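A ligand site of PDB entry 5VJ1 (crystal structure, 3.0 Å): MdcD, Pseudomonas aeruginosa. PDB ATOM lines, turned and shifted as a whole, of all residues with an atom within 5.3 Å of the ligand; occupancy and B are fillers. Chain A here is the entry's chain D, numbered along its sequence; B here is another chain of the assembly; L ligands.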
ATOM      1  N   ALA A  79      15.763  18.790   2.414  1.00  0.00           N
ATOM      2  CA  ALA A  79      15.113  17.490   2.537  1.00  0.00           C
ATOM      3  C   ALA A  79      15.239  16.903   3.959  1.00  0.00           C
ATOM      4  O   ALA A  79      14.280  16.333   4.501  1.00  0.00           O
ATOM      5  CB  ALA A  79      15.679  16.555   1.534  1.00  0.00           C
ATOM      6  N   GLN A  81      15.213  17.003   7.751  1.00  0.00           N
ATOM      7  CA  GLN A  81      14.613  17.704   8.884  1.00  0.00           C
ATOM      8  C   GLN A  81      14.280  19.136   8.545  1.00  0.00           C
ATOM      9  O   GLN A  81      14.407  20.018   9.391  1.00  0.00           O
ATOM     10  CB  GLN A  81      15.535  17.622  10.103  1.00  0.00           C
ATOM     11  CG  GLN A  81      15.827  16.183  10.499  1.00  0.00           C
ATOM     12  CD  GLN A  81      14.686  15.516  11.255  1.00  0.00           C
ATOM     13  OE1 GLN A  81      13.512  15.611  10.881  1.00  0.00           O
ATOM     14  NE2 GLN A  81      15.043  14.806  12.302  1.00  0.00           N
ATOM     15  N   GLY A  82      13.828  19.348   7.312  1.00  0.00           N
ATOM     16  CA  GLY A  82      13.448  20.663   6.819  1.00  0.00           C
ATOM     17  C   GLY A  82      14.550  21.700   6.713  1.00  0.00           C
ATOM     18  O   GLY A  82      14.286  22.850   6.422  1.00  0.00           O
ATOM     19  N   SER A  84      16.575  22.061   9.272  1.00  0.00           N
ATOM     20  CA  SER A  84      16.803  22.392  10.668  1.00  0.00           C
ATOM     21  C   SER A  84      18.245  22.204  11.100  1.00  0.00           C
ATOM     22  O   SER A  84      18.862  21.179  10.803  1.00  0.00           O
ATOM     23  CB  SER A  84      15.932  21.527  11.558  1.00  0.00           C
ATOM     24  OG  SER A  84      14.577  21.740  11.297  1.00  0.00           O
ATOM     25  N   THR A 118      16.382  26.562   5.246  1.00  0.00           N
ATOM     26  CA  THR A 118      16.296  26.091   6.609  1.00  0.00           C
ATOM     27  C   THR A 118      15.003  26.436   7.312  1.00  0.00           C
ATOM     28  O   THR A 118      14.310  27.369   6.946  1.00  0.00           O
ATOM     29  CB  THR A 118      17.497  26.668   7.424  1.00  0.00           C
ATOM     30  OG1 THR A 118      17.422  26.224   8.790  1.00  0.00           O
ATOM     31  CG2 THR A 118      17.472  28.183   7.387  1.00  0.00           C
ATOM     32  N   GLY A 119      14.693  25.657   8.335  1.00  0.00           N
ATOM     33  CA  GLY A 119      13.507  25.866   9.130  1.00  0.00           C
ATOM     34  C   GLY A 119      13.902  26.366  10.503  1.00  0.00           C
ATOM     35  O   GLY A 119      13.105  26.330  11.432  1.00  0.00           O
ATOM     36  N   GLY A 120      15.147  26.810  10.623  1.00  0.00           N
ATOM     37  CA  GLY A 120      15.631  27.401  11.853  1.00  0.00           C
ATOM     38  C   GLY A 120      16.233  26.351  12.759  1.00  0.00           C
ATOM     39  O   GLY A 120      16.853  25.392  12.271  1.00  0.00           O
ATOM     40  N   VAL A 121      16.061  26.541  14.061  1.00  0.00           N
ATOM     41  CA  VAL A 121      16.538  25.557  15.025  1.00  0.00           C
ATOM     42  C   VAL A 121      15.803  24.221  14.856  1.00  0.00           C
ATOM     43  O   VAL A 121      14.576  24.182  14.724  1.00  0.00           O
ATOM     44  CB  VAL A 121      16.346  26.039  16.447  1.00  0.00           C
ATOM     45  CG1 VAL A 121      16.842  25.010  17.420  1.00  0.00           C
ATOM     46  CG2 VAL A 121      17.069  27.346  16.665  1.00  0.00           C
ATOM     47  N   ARG A 122      16.561  23.128  14.870  1.00  0.00           N
ATOM     48  CA  ARG A 122      15.954  21.807  14.892  1.00  0.00           C
ATOM     49  C   ARG A 122      15.327  21.544  16.280  1.00  0.00           C
ATOM     50  O   ARG A 122      16.032  21.301  17.278  1.00  0.00           O
ATOM     51  CB  ARG A 122      16.997  20.744  14.563  1.00  0.00           C
ATOM     52  CG  ARG A 122      16.442  19.361  14.316  1.00  0.00           C
ATOM     53  CD  ARG A 122      17.573  18.365  14.015  1.00  0.00           C
ATOM     54  NE  ARG A 122      18.423  18.743  12.889  1.00  0.00           N
ATOM     55  CZ  ARG A 122      19.600  18.186  12.628  1.00  0.00           C
ATOM     56  NH1 ARG A 122      20.058  17.214  13.405  1.00  0.00           N
ATOM     57  NH2 ARG A 122      20.336  18.583  11.580  1.00  0.00           N
ATOM     58  N   LEU A 123      13.995  21.644  16.362  1.00  0.00           N
ATOM     59  CA  LEU A 123      13.310  21.523  17.640  1.00  0.00           C
ATOM     60  C   LEU A 123      13.619  20.237  18.401  1.00  0.00           C
ATOM     61  O   LEU A 123      13.305  20.129  19.579  1.00  0.00           O
ATOM     62  CB  LEU A 123      11.807  21.671  17.440  1.00  0.00           C
ATOM     63  CG  LEU A 123      11.445  23.014  16.815  1.00  0.00           C
ATOM     64  CD1 LEU A 123      10.044  22.981  16.296  1.00  0.00           C
ATOM     65  CD2 LEU A 123      11.593  24.076  17.865  1.00  0.00           C
ATOM     66  N   GLN A 124      14.221  19.255  17.715  1.00  0.00           N
ATOM     67  CA  GLN A 124      14.574  17.984  18.334  1.00  0.00           C
ATOM     68  C   GLN A 124      15.938  18.056  18.971  1.00  0.00           C
ATOM     69  O   GLN A 124      16.401  17.097  19.571  1.00  0.00           O
ATOM     70  CB  GLN A 124      14.586  16.824  17.333  1.00  0.00           C
ATOM     71  CG  GLN A 124      13.237  16.428  16.768  1.00  0.00           C
ATOM     72  CD  GLN A 124      12.969  17.097  15.465  1.00  0.00           C
ATOM     73  OE1 GLN A 124      13.695  17.999  15.055  1.00  0.00           O
ATOM     74  NE2 GLN A 124      11.925  16.646  14.771  1.00  0.00           N
ATOM     75  N   PRO A 156      13.042  25.443  -2.074  1.00  0.00           N
ATOM     76  CA  PRO A 156      11.620  25.524  -1.700  1.00  0.00           C
ATOM     77  C   PRO A 156      11.319  25.865  -0.235  1.00  0.00           C
ATOM     78  O   PRO A 156      10.465  26.717   0.000  1.00  0.00           O
ATOM     79  CB  PRO A 156      11.117  24.120  -2.009  1.00  0.00           C
ATOM     80  CG  PRO A 156      12.325  23.257  -1.843  1.00  0.00           C
ATOM     81  CD  PRO A 156      13.427  24.070  -2.433  1.00  0.00           C
ATOM     82  N   VAL A 157      11.964  25.189   0.725  1.00  0.00           N
ATOM     83  CA  VAL A 157      11.708  25.451   2.142  1.00  0.00           C
ATOM     84  C   VAL A 157      11.739  26.932   2.499  1.00  0.00           C
ATOM     85  O   VAL A 157      10.862  27.419   3.212  1.00  0.00           O
ATOM     86  CB  VAL A 157      12.718  24.737   3.035  1.00  0.00           C
ATOM     87  CG1 VAL A 157      12.515  25.151   4.484  1.00  0.00           C
ATOM     88  CG2 VAL A 157      12.577  23.246   2.886  1.00  0.00           C
ATOM     89  N   PHE A 160      13.795  30.391   7.701  1.00  0.00           N
ATOM     90  CA  PHE A 160      13.014  30.792   8.848  1.00  0.00           C
ATOM     91  C   PHE A 160      13.778  30.656  10.157  1.00  0.00           C
ATOM     92  O   PHE A 160      14.912  30.157  10.195  1.00  0.00           O
ATOM     93  CB  PHE A 160      11.739  29.967   8.901  1.00  0.00           C
ATOM     94  CG  PHE A 160      10.803  30.225   7.766  1.00  0.00           C
ATOM     95  CD1 PHE A 160       9.655  30.970   7.951  1.00  0.00           C
ATOM     96  CD2 PHE A 160      11.063  29.723   6.486  1.00  0.00           C
ATOM     97  CE1 PHE A 160       8.774  31.211   6.887  1.00  0.00           C
ATOM     98  CE2 PHE A 160      10.191  29.968   5.420  1.00  0.00           C
ATOM     99  CZ  PHE A 160       9.061  30.701   5.617  1.00  0.00           C
ATOM    100  N   GLY A 161      13.140  31.109  11.246  1.00  0.00           N
ATOM    101  CA  GLY A 161      13.662  30.938  12.586  1.00  0.00           C
ATOM    102  C   GLY A 161      14.935  31.718  12.832  1.00  0.00           C
ATOM    103  O   GLY A 161      15.116  32.818  12.284  1.00  0.00           O
ATOM    104  N   GLY A 162      15.821  31.166  13.648  1.00  0.00           N
ATOM    105  CA  GLY A 162      17.062  31.827  13.986  1.00  0.00           C
ATOM    106  C   GLY A 162      17.920  32.209  12.797  1.00  0.00           C
ATOM    107  O   GLY A 162      18.654  33.201  12.849  1.00  0.00           O
ATOM    108  N   ARG A 180      11.043  32.161   0.703  1.00  0.00           N
ATOM    109  CA  ARG A 180      10.400  32.981   1.688  1.00  0.00           C
ATOM    110  C   ARG A 180      11.498  33.320   2.660  1.00  0.00           C
ATOM    111  O   ARG A 180      12.492  32.588   2.734  1.00  0.00           O
ATOM    112  CB  ARG A 180       9.242  32.256   2.408  1.00  0.00           C
ATOM    113  CG  ARG A 180       8.183  31.596   1.526  1.00  0.00           C
ATOM    114  CD  ARG A 180       8.297  30.076   1.618  1.00  0.00           C
ATOM    115  NE  ARG A 180       7.170  29.447   2.302  1.00  0.00           N
ATOM    116  CZ  ARG A 180       7.189  28.180   2.726  1.00  0.00           C
ATOM    117  NH1 ARG A 180       8.275  27.452   2.543  1.00  0.00           N
ATOM    118  NH2 ARG A 180       6.130  27.646   3.341  1.00  0.00           N
ATOM    119  N   LEU A 183      10.586  35.365  10.098  1.00  0.00           N
ATOM    120  CA  LEU A 183      11.135  34.961  11.375  1.00  0.00           C
ATOM    121  C   LEU A 183      10.439  33.698  11.804  1.00  0.00           C
ATOM    122  O   LEU A 183      11.096  32.674  12.008  1.00  0.00           O
ATOM    123  CB  LEU A 183      10.967  36.054  12.448  1.00  0.00           C
ATOM    124  CG  LEU A 183      11.481  35.654  13.831  1.00  0.00           C
ATOM    125  CD1 LEU A 183      12.942  35.252  13.723  1.00  0.00           C
ATOM    126  CD2 LEU A 183      11.308  36.811  14.787  1.00  0.00           C
ATOM    127  N   ASN A 184       9.127  33.787  11.959  1.00  0.00           N
ATOM    128  CA  ASN A 184       8.312  32.646  12.371  1.00  0.00           C
ATOM    129  C   ASN A 184       7.548  32.003  11.231  1.00  0.00           C
ATOM    130  O   ASN A 184       6.891  32.706  10.441  1.00  0.00           O
ATOM    131  CB  ASN A 184       7.338  33.078  13.436  1.00  0.00           C
ATOM    132  CG  ASN A 184       8.003  33.533  14.690  1.00  0.00           C
ATOM    133  OD1 ASN A 184       7.636  34.570  15.228  1.00  0.00           O
ATOM    134  ND2 ASN A 184       8.946  32.726  15.199  1.00  0.00           N
ATOM    135  N   GLY A 185       7.596  30.680  11.170  1.00  0.00           N
ATOM    136  CA  GLY A 185       6.897  29.950  10.127  1.00  0.00           C
ATOM    137  C   GLY A 185       5.403  30.119  10.250  1.00  0.00           C
ATOM    138  O   GLY A 185       4.893  30.244  11.362  1.00  0.00           O
ATOM    139  N   PRO A 186       4.700  30.101   9.105  1.00  0.00           N
ATOM    140  CA  PRO A 186       3.266  30.384   9.042  1.00  0.00           C
ATOM    141  C   PRO A 186       2.443  29.598  10.064  1.00  0.00           C
ATOM    142  O   PRO A 186       1.608  30.228  10.729  1.00  0.00           O
ATOM    143  CB  PRO A 186       2.906  29.988   7.611  1.00  0.00           C
ATOM    144  CG  PRO A 186       4.140  30.296   6.857  1.00  0.00           C
ATOM    145  CD  PRO A 186       5.235  29.812   7.771  1.00  0.00           C
ATOM    146  N   GLN A 187       2.694  28.305  10.214  1.00  0.00           N
ATOM    147  CA  GLN A 187       1.926  27.524  11.188  1.00  0.00           C
ATOM    148  C   GLN A 187       2.155  28.047  12.602  1.00  0.00           C
ATOM    149  O   GLN A 187       1.189  28.237  13.361  1.00  0.00           O
ATOM    150  CB  GLN A 187       2.300  26.045  11.121  1.00  0.00           C
ATOM    151  CG  GLN A 187       2.255  25.467   9.744  1.00  0.00           C
ATOM    152  CD  GLN A 187       2.151  23.953   9.741  1.00  0.00           C
ATOM    153  OE1 GLN A 187       1.886  23.342  10.783  1.00  0.00           O
ATOM    154  NE2 GLN A 187       2.345  23.343   8.575  1.00  0.00           N
ATOM    155  N   VAL A 188       3.422  28.277  12.954  1.00  0.00           N
ATOM    156  CA  VAL A 188       3.779  28.723  14.301  1.00  0.00           C
ATOM    157  C   VAL A 188       3.049  30.015  14.692  1.00  0.00           C
ATOM    158  O   VAL A 188       2.629  30.176  15.838  1.00  0.00           O
ATOM    159  CB  VAL A 188       5.284  28.942  14.438  1.00  0.00           C
ATOM    160  CG1 VAL A 188       5.622  29.167  15.900  1.00  0.00           C
ATOM    161  CG2 VAL A 188       6.050  27.740  13.910  1.00  0.00           C
ATOM    162  N   ARG A 203      -1.433  30.004   0.898  1.00  0.00           N
ATOM    163  CA  ARG A 203      -0.113  30.144   0.288  1.00  0.00           C
ATOM    164  C   ARG A 203       0.164  31.447  -0.471  1.00  0.00           C
ATOM    165  O   ARG A 203       1.236  32.010  -0.311  1.00  0.00           O
ATOM    166  CB  ARG A 203       0.136  28.949  -0.636  1.00  0.00           C
ATOM    167  CG  ARG A 203       0.223  27.679   0.143  1.00  0.00           C
ATOM    168  CD  ARG A 203       0.404  26.521  -0.772  1.00  0.00           C
ATOM    169  NE  ARG A 203       1.664  26.592  -1.496  1.00  0.00           N
ATOM    170  CZ  ARG A 203       2.834  26.218  -0.995  1.00  0.00           C
ATOM    171  NH1 ARG A 203       2.902  25.735   0.233  1.00  0.00           N
ATOM    172  NH2 ARG A 203       3.931  26.299  -1.747  1.00  0.00           N
ATOM    173  N   SER B 158      13.970  31.459  21.784  1.00  0.00           N
ATOM    174  CA  SER B 158      14.196  31.613  20.356  1.00  0.00           C
ATOM    175  C   SER B 158      14.889  32.887  19.936  1.00  0.00           C
ATOM    176  O   SER B 158      15.931  33.240  20.467  1.00  0.00           O
ATOM    177  CB  SER B 158      12.880  31.528  19.594  1.00  0.00           C
ATOM    178  OG  SER B 158      13.121  31.341  18.202  1.00  0.00           O
ATOM    179  N   ALA B 183      13.609  27.195  22.119  1.00  0.00           N
ATOM    180  CA  ALA B 183      13.407  27.877  20.847  1.00  0.00           C
ATOM    181  C   ALA B 183      11.949  27.950  20.433  1.00  0.00           C
ATOM    182  O   ALA B 183      11.626  28.593  19.420  1.00  0.00           O
ATOM    183  CB  ALA B 183      14.215  27.220  19.747  1.00  0.00           C
ATOM    184  N   MET B 184      11.068  27.325  21.207  1.00  0.00           N
ATOM    185  CA  MET B 184       9.655  27.319  20.858  1.00  0.00           C
ATOM    186  C   MET B 184       8.789  26.766  21.984  1.00  0.00           C
ATOM    187  O   MET B 184       9.227  25.916  22.746  1.00  0.00           O
ATOM    188  CB  MET B 184       9.436  26.495  19.595  1.00  0.00           C
ATOM    189  CG  MET B 184       8.063  26.588  19.034  1.00  0.00           C
ATOM    190  SD  MET B 184       8.004  25.826  17.421  1.00  0.00           S
ATOM    191  CE  MET B 184       8.694  27.078  16.357  1.00  0.00           C
ATOM    192  N   ILE B 192       4.852  21.386  14.682  1.00  0.00           N
ATOM    193  CA  ILE B 192       5.845  21.381  13.599  1.00  0.00           C
ATOM    194  C   ILE B 192       6.555  20.036  13.450  1.00  0.00           C
ATOM    195  O   ILE B 192       6.732  19.517  12.336  1.00  0.00           O
ATOM    196  CB  ILE B 192       6.904  22.462  13.827  1.00  0.00           C
ATOM    197  CG1 ILE B 192       6.265  23.852  13.754  1.00  0.00           C
ATOM    198  CG2 ILE B 192       8.015  22.312  12.819  1.00  0.00           C
ATOM    199  CD1 ILE B 192       5.682  24.191  12.391  1.00  0.00           C
ATOM    200  N   THR B 193       6.971  19.529  14.609  1.00  0.00           N
ATOM    201  CA  THR B 193       7.694  18.272  14.778  1.00  0.00           C
ATOM    202  C   THR B 193       6.845  17.014  14.468  1.00  0.00           C
ATOM    203  O   THR B 193       7.368  16.023  13.925  1.00  0.00           O
ATOM    204  CB  THR B 193       8.226  18.204  16.227  1.00  0.00           C
ATOM    205  OG1 THR B 193       9.131  19.280  16.440  1.00  0.00           O
ATOM    206  CG2 THR B 193       8.946  16.920  16.496  1.00  0.00           C
HETATM  207  N1  LIG L   1      12.618  21.571  13.449  1.00  0.00           N
HETATM  208  C1  LIG L   1      12.448  20.333  12.998  1.00  0.00           C
HETATM  209  N2  LIG L   1      11.876  20.092  11.830  1.00  0.00           N
HETATM  210  C2  LIG L   1      11.448  21.101  11.061  1.00  0.00           C
HETATM  211  C3  LIG L   1      11.609  22.410  11.497  1.00  0.00           C
HETATM  212  C4  LIG L   1      12.224  22.625  12.719  1.00  0.00           C
HETATM  213  N3  LIG L   1      12.438  23.860  13.166  1.00  0.00           N
HETATM  214  N4  LIG L   1      11.104  23.208  10.557  1.00  0.00           N
HETATM  215  C5  LIG L   1      10.640  22.439   9.573  1.00  0.00           C
HETATM  216  N5  LIG L   1      10.841  21.154   9.880  1.00  0.00           N
HETATM  217  C6  LIG L   1      10.448  19.990   9.052  1.00  0.00           C
HETATM  218  C7  LIG L   1       9.031  19.512   9.337  1.00  0.00           C
HETATM  219  O1  LIG L   1       9.015  18.706  10.524  1.00  0.00           O
HETATM  220  C8  LIG L   1       8.731  18.659   8.109  1.00  0.00           C
HETATM  221  O2  LIG L   1       9.101  17.301   8.397  1.00  0.00           O
HETATM  222  P1  LIG L   1       9.010  16.150   7.279  1.00  0.00           P
HETATM  223  O3  LIG L   1       7.670  16.099   6.635  1.00  0.00           O
HETATM  224  O4  LIG L   1       9.373  14.789   8.042  1.00  0.00           O
HETATM  225  O5  LIG L   1      10.190  16.422   6.218  1.00  0.00           O
HETATM  226  C9  LIG L   1       9.662  19.238   7.032  1.00  0.00           C
HETATM  227  O6  LIG L   1      10.392  20.313   7.653  1.00  0.00           O
HETATM  228  C10 LIG L   1       8.834  19.747   5.850  1.00  0.00           C
HETATM  229  O7  LIG L   1       8.182  20.986   6.131  1.00  0.00           O
HETATM  230  P2  LIG L   1       6.797  21.376   5.400  1.00  0.00           P
HETATM  231  O8  LIG L   1       5.892  21.963   6.412  1.00  0.00           O
HETATM  232  O9  LIG L   1       6.355  20.184   4.655  1.00  0.00           O
HETATM  233  O10 LIG L   1       7.227  22.512   4.336  1.00  0.00           O
HETATM  234  P3  LIG L   1       6.552  23.980   4.351  1.00  0.00           P
HETATM  235  O11 LIG L   1       5.079  23.840   4.440  1.00  0.00           O
HETATM  236  O12 LIG L   1       7.112  24.739   3.216  1.00  0.00           O
HETATM  237  O13 LIG L   1       7.099  24.595   5.734  1.00  0.00           O
HETATM  238  C11 LIG L   1       8.579  25.940   7.139  1.00  0.00           C
HETATM  239  C12 LIG L   1       8.397  25.190   5.824  1.00  0.00           C
HETATM  240  C13 LIG L   1      10.063  25.970   7.506  1.00  0.00           C
HETATM  241  C14 LIG L   1       8.064  27.371   6.992  1.00  0.00           C
HETATM  242  C15 LIG L   1       7.800  25.225   8.253  1.00  0.00           C
HETATM  243  O14 LIG L   1       8.363  23.929   8.477  1.00  0.00           O
HETATM  244  C16 LIG L   1       7.814  26.030   9.551  1.00  0.00           C
HETATM  245  O15 LIG L   1       6.829  26.687   9.884  1.00  0.00           O
HETATM  246  N6  LIG L   1       8.917  25.926  10.284  1.00  0.00           N
HETATM  247  C17 LIG L   1       9.051  26.555  11.600  1.00  0.00           C
HETATM  248  C18 LIG L   1      10.281  27.456  11.647  1.00  0.00           C
HETATM  249  C19 LIG L   1      10.355  28.257  12.960  1.00  0.00           C
HETATM  250  O16 LIG L   1       9.438  29.010  13.286  1.00  0.00           O
HETATM  251  N7  LIG L   1      11.445  28.047  13.688  1.00  0.00           N
HETATM  252  C20 LIG L   1      11.444  28.166  15.155  1.00  0.00           C
HETATM  253  C21 LIG L   1      12.754  27.649  15.737  1.00  0.00           C
HETATM  254  S1  LIG L   1      14.008  28.968  16.005  1.00  0.00           S
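Residues that only touch the ligand: Gly 82 (3.2 Å), Met 184 of chain B (3.2 Å), Gln 124 (3.4 Å), Gln 81 (3.5 Å), Arg 122 (3.6 Å), Val 188 (3.7 Å), Phe 160 (3.7 Å), Gly 161 (3.8 Å), Pro 186 (3.8 Å), Asn 184 of chain A (3.9 Å), Ala 183 of chain B (3.97 Å) and Val 157 (3.98 Å). Hydrophobic or aromatic side chains that line the ligand: Val 121, Leu 123, Val 157, Phe 160, Pro 186, Val 188, Met 184 of chain B and Ile 192 of chain B. Within 4 Å of the ligand: Gln 81, Gly 82, Ser 84, Gly 119, Val 121, Arg 122, Leu 123, Gln 124, Val 157, Phe 160, Gly 161, Gly 162, Arg 180, Asn 184 of chain A, Gly 185, Pro 186, Val 188, Ser 158 of chain B, Ala 183 of chain B, Met 184 of chain B and Ile 192 of chain B. The nearest printed residue that does not touch the ligand is Leu 183 of chain A (4.2 Å).
The backbone NH (N) of Val 121 lies close to a sulfur (S1) of the ligand, 3.7 Å away. N3 of the ligand sits at hydrogen-bond distance from O of Val 121. OG of Ser 84 sits close to N1 of the ligand. O1 of the ligand is in hydrogen-bond range of O of Ile 192 of chain B (3.0 Å). NH1 of Arg 180 is in salt-bridge range of O12 of the ligand, 3.0 Å away. O of Gly 119 lies close to N3 of the ligand (3.1 Å). The backbone NH (N) of Leu 123 lies within hydrogen-bond range of a nitrogen (N1) of the ligand (3.2 Å). The backbone NH (N) of Gly 185 lies within hydrogen-bond range of an oxygen (O16) of the ligand, at 3.3 Å. The side-chain hydroxyl (OG) of Ser 158 of chain B lies close to a sulfur (S1) of the ligand. The backbone NH (N) of Gly 162 sits close to a sulfur (S1) of the ligand (3.7 Å).
The side-chain hydroxyl (OG) of Ser 84 is in hydrogen-bond range of the backbone carbonyl oxygen (O) of Gln 81 (2.6 Å). O of Ser 84 lies within hydrogen-bond range of NH2 of Arg 122 (3.1 Å). The guanidinium group (NH1) of Arg 180 is in hydrogen-bond range of the backbone carbonyl oxygen (O) of Val 157 (2.7 Å). The backbone carbonyl oxygen of Pro 156 lies within hydrogen-bond range of the guanidinium group of Arg 180, 3.4 Å away. O of Ala 183 of chain B lies close to OG of Ser 158 of chain B, 3.4 Å away. The backbone carbonyl oxygen of Thr 118 is in hydrogen-bond range of the backbone NH of Phe 160. O of Phe 160 lies close to N of Gly 120 (3.4 Å). The backbone NH of Gly 161 is in hydrogen-bond range of the backbone carbonyl oxygen of Leu 183 of chain A.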
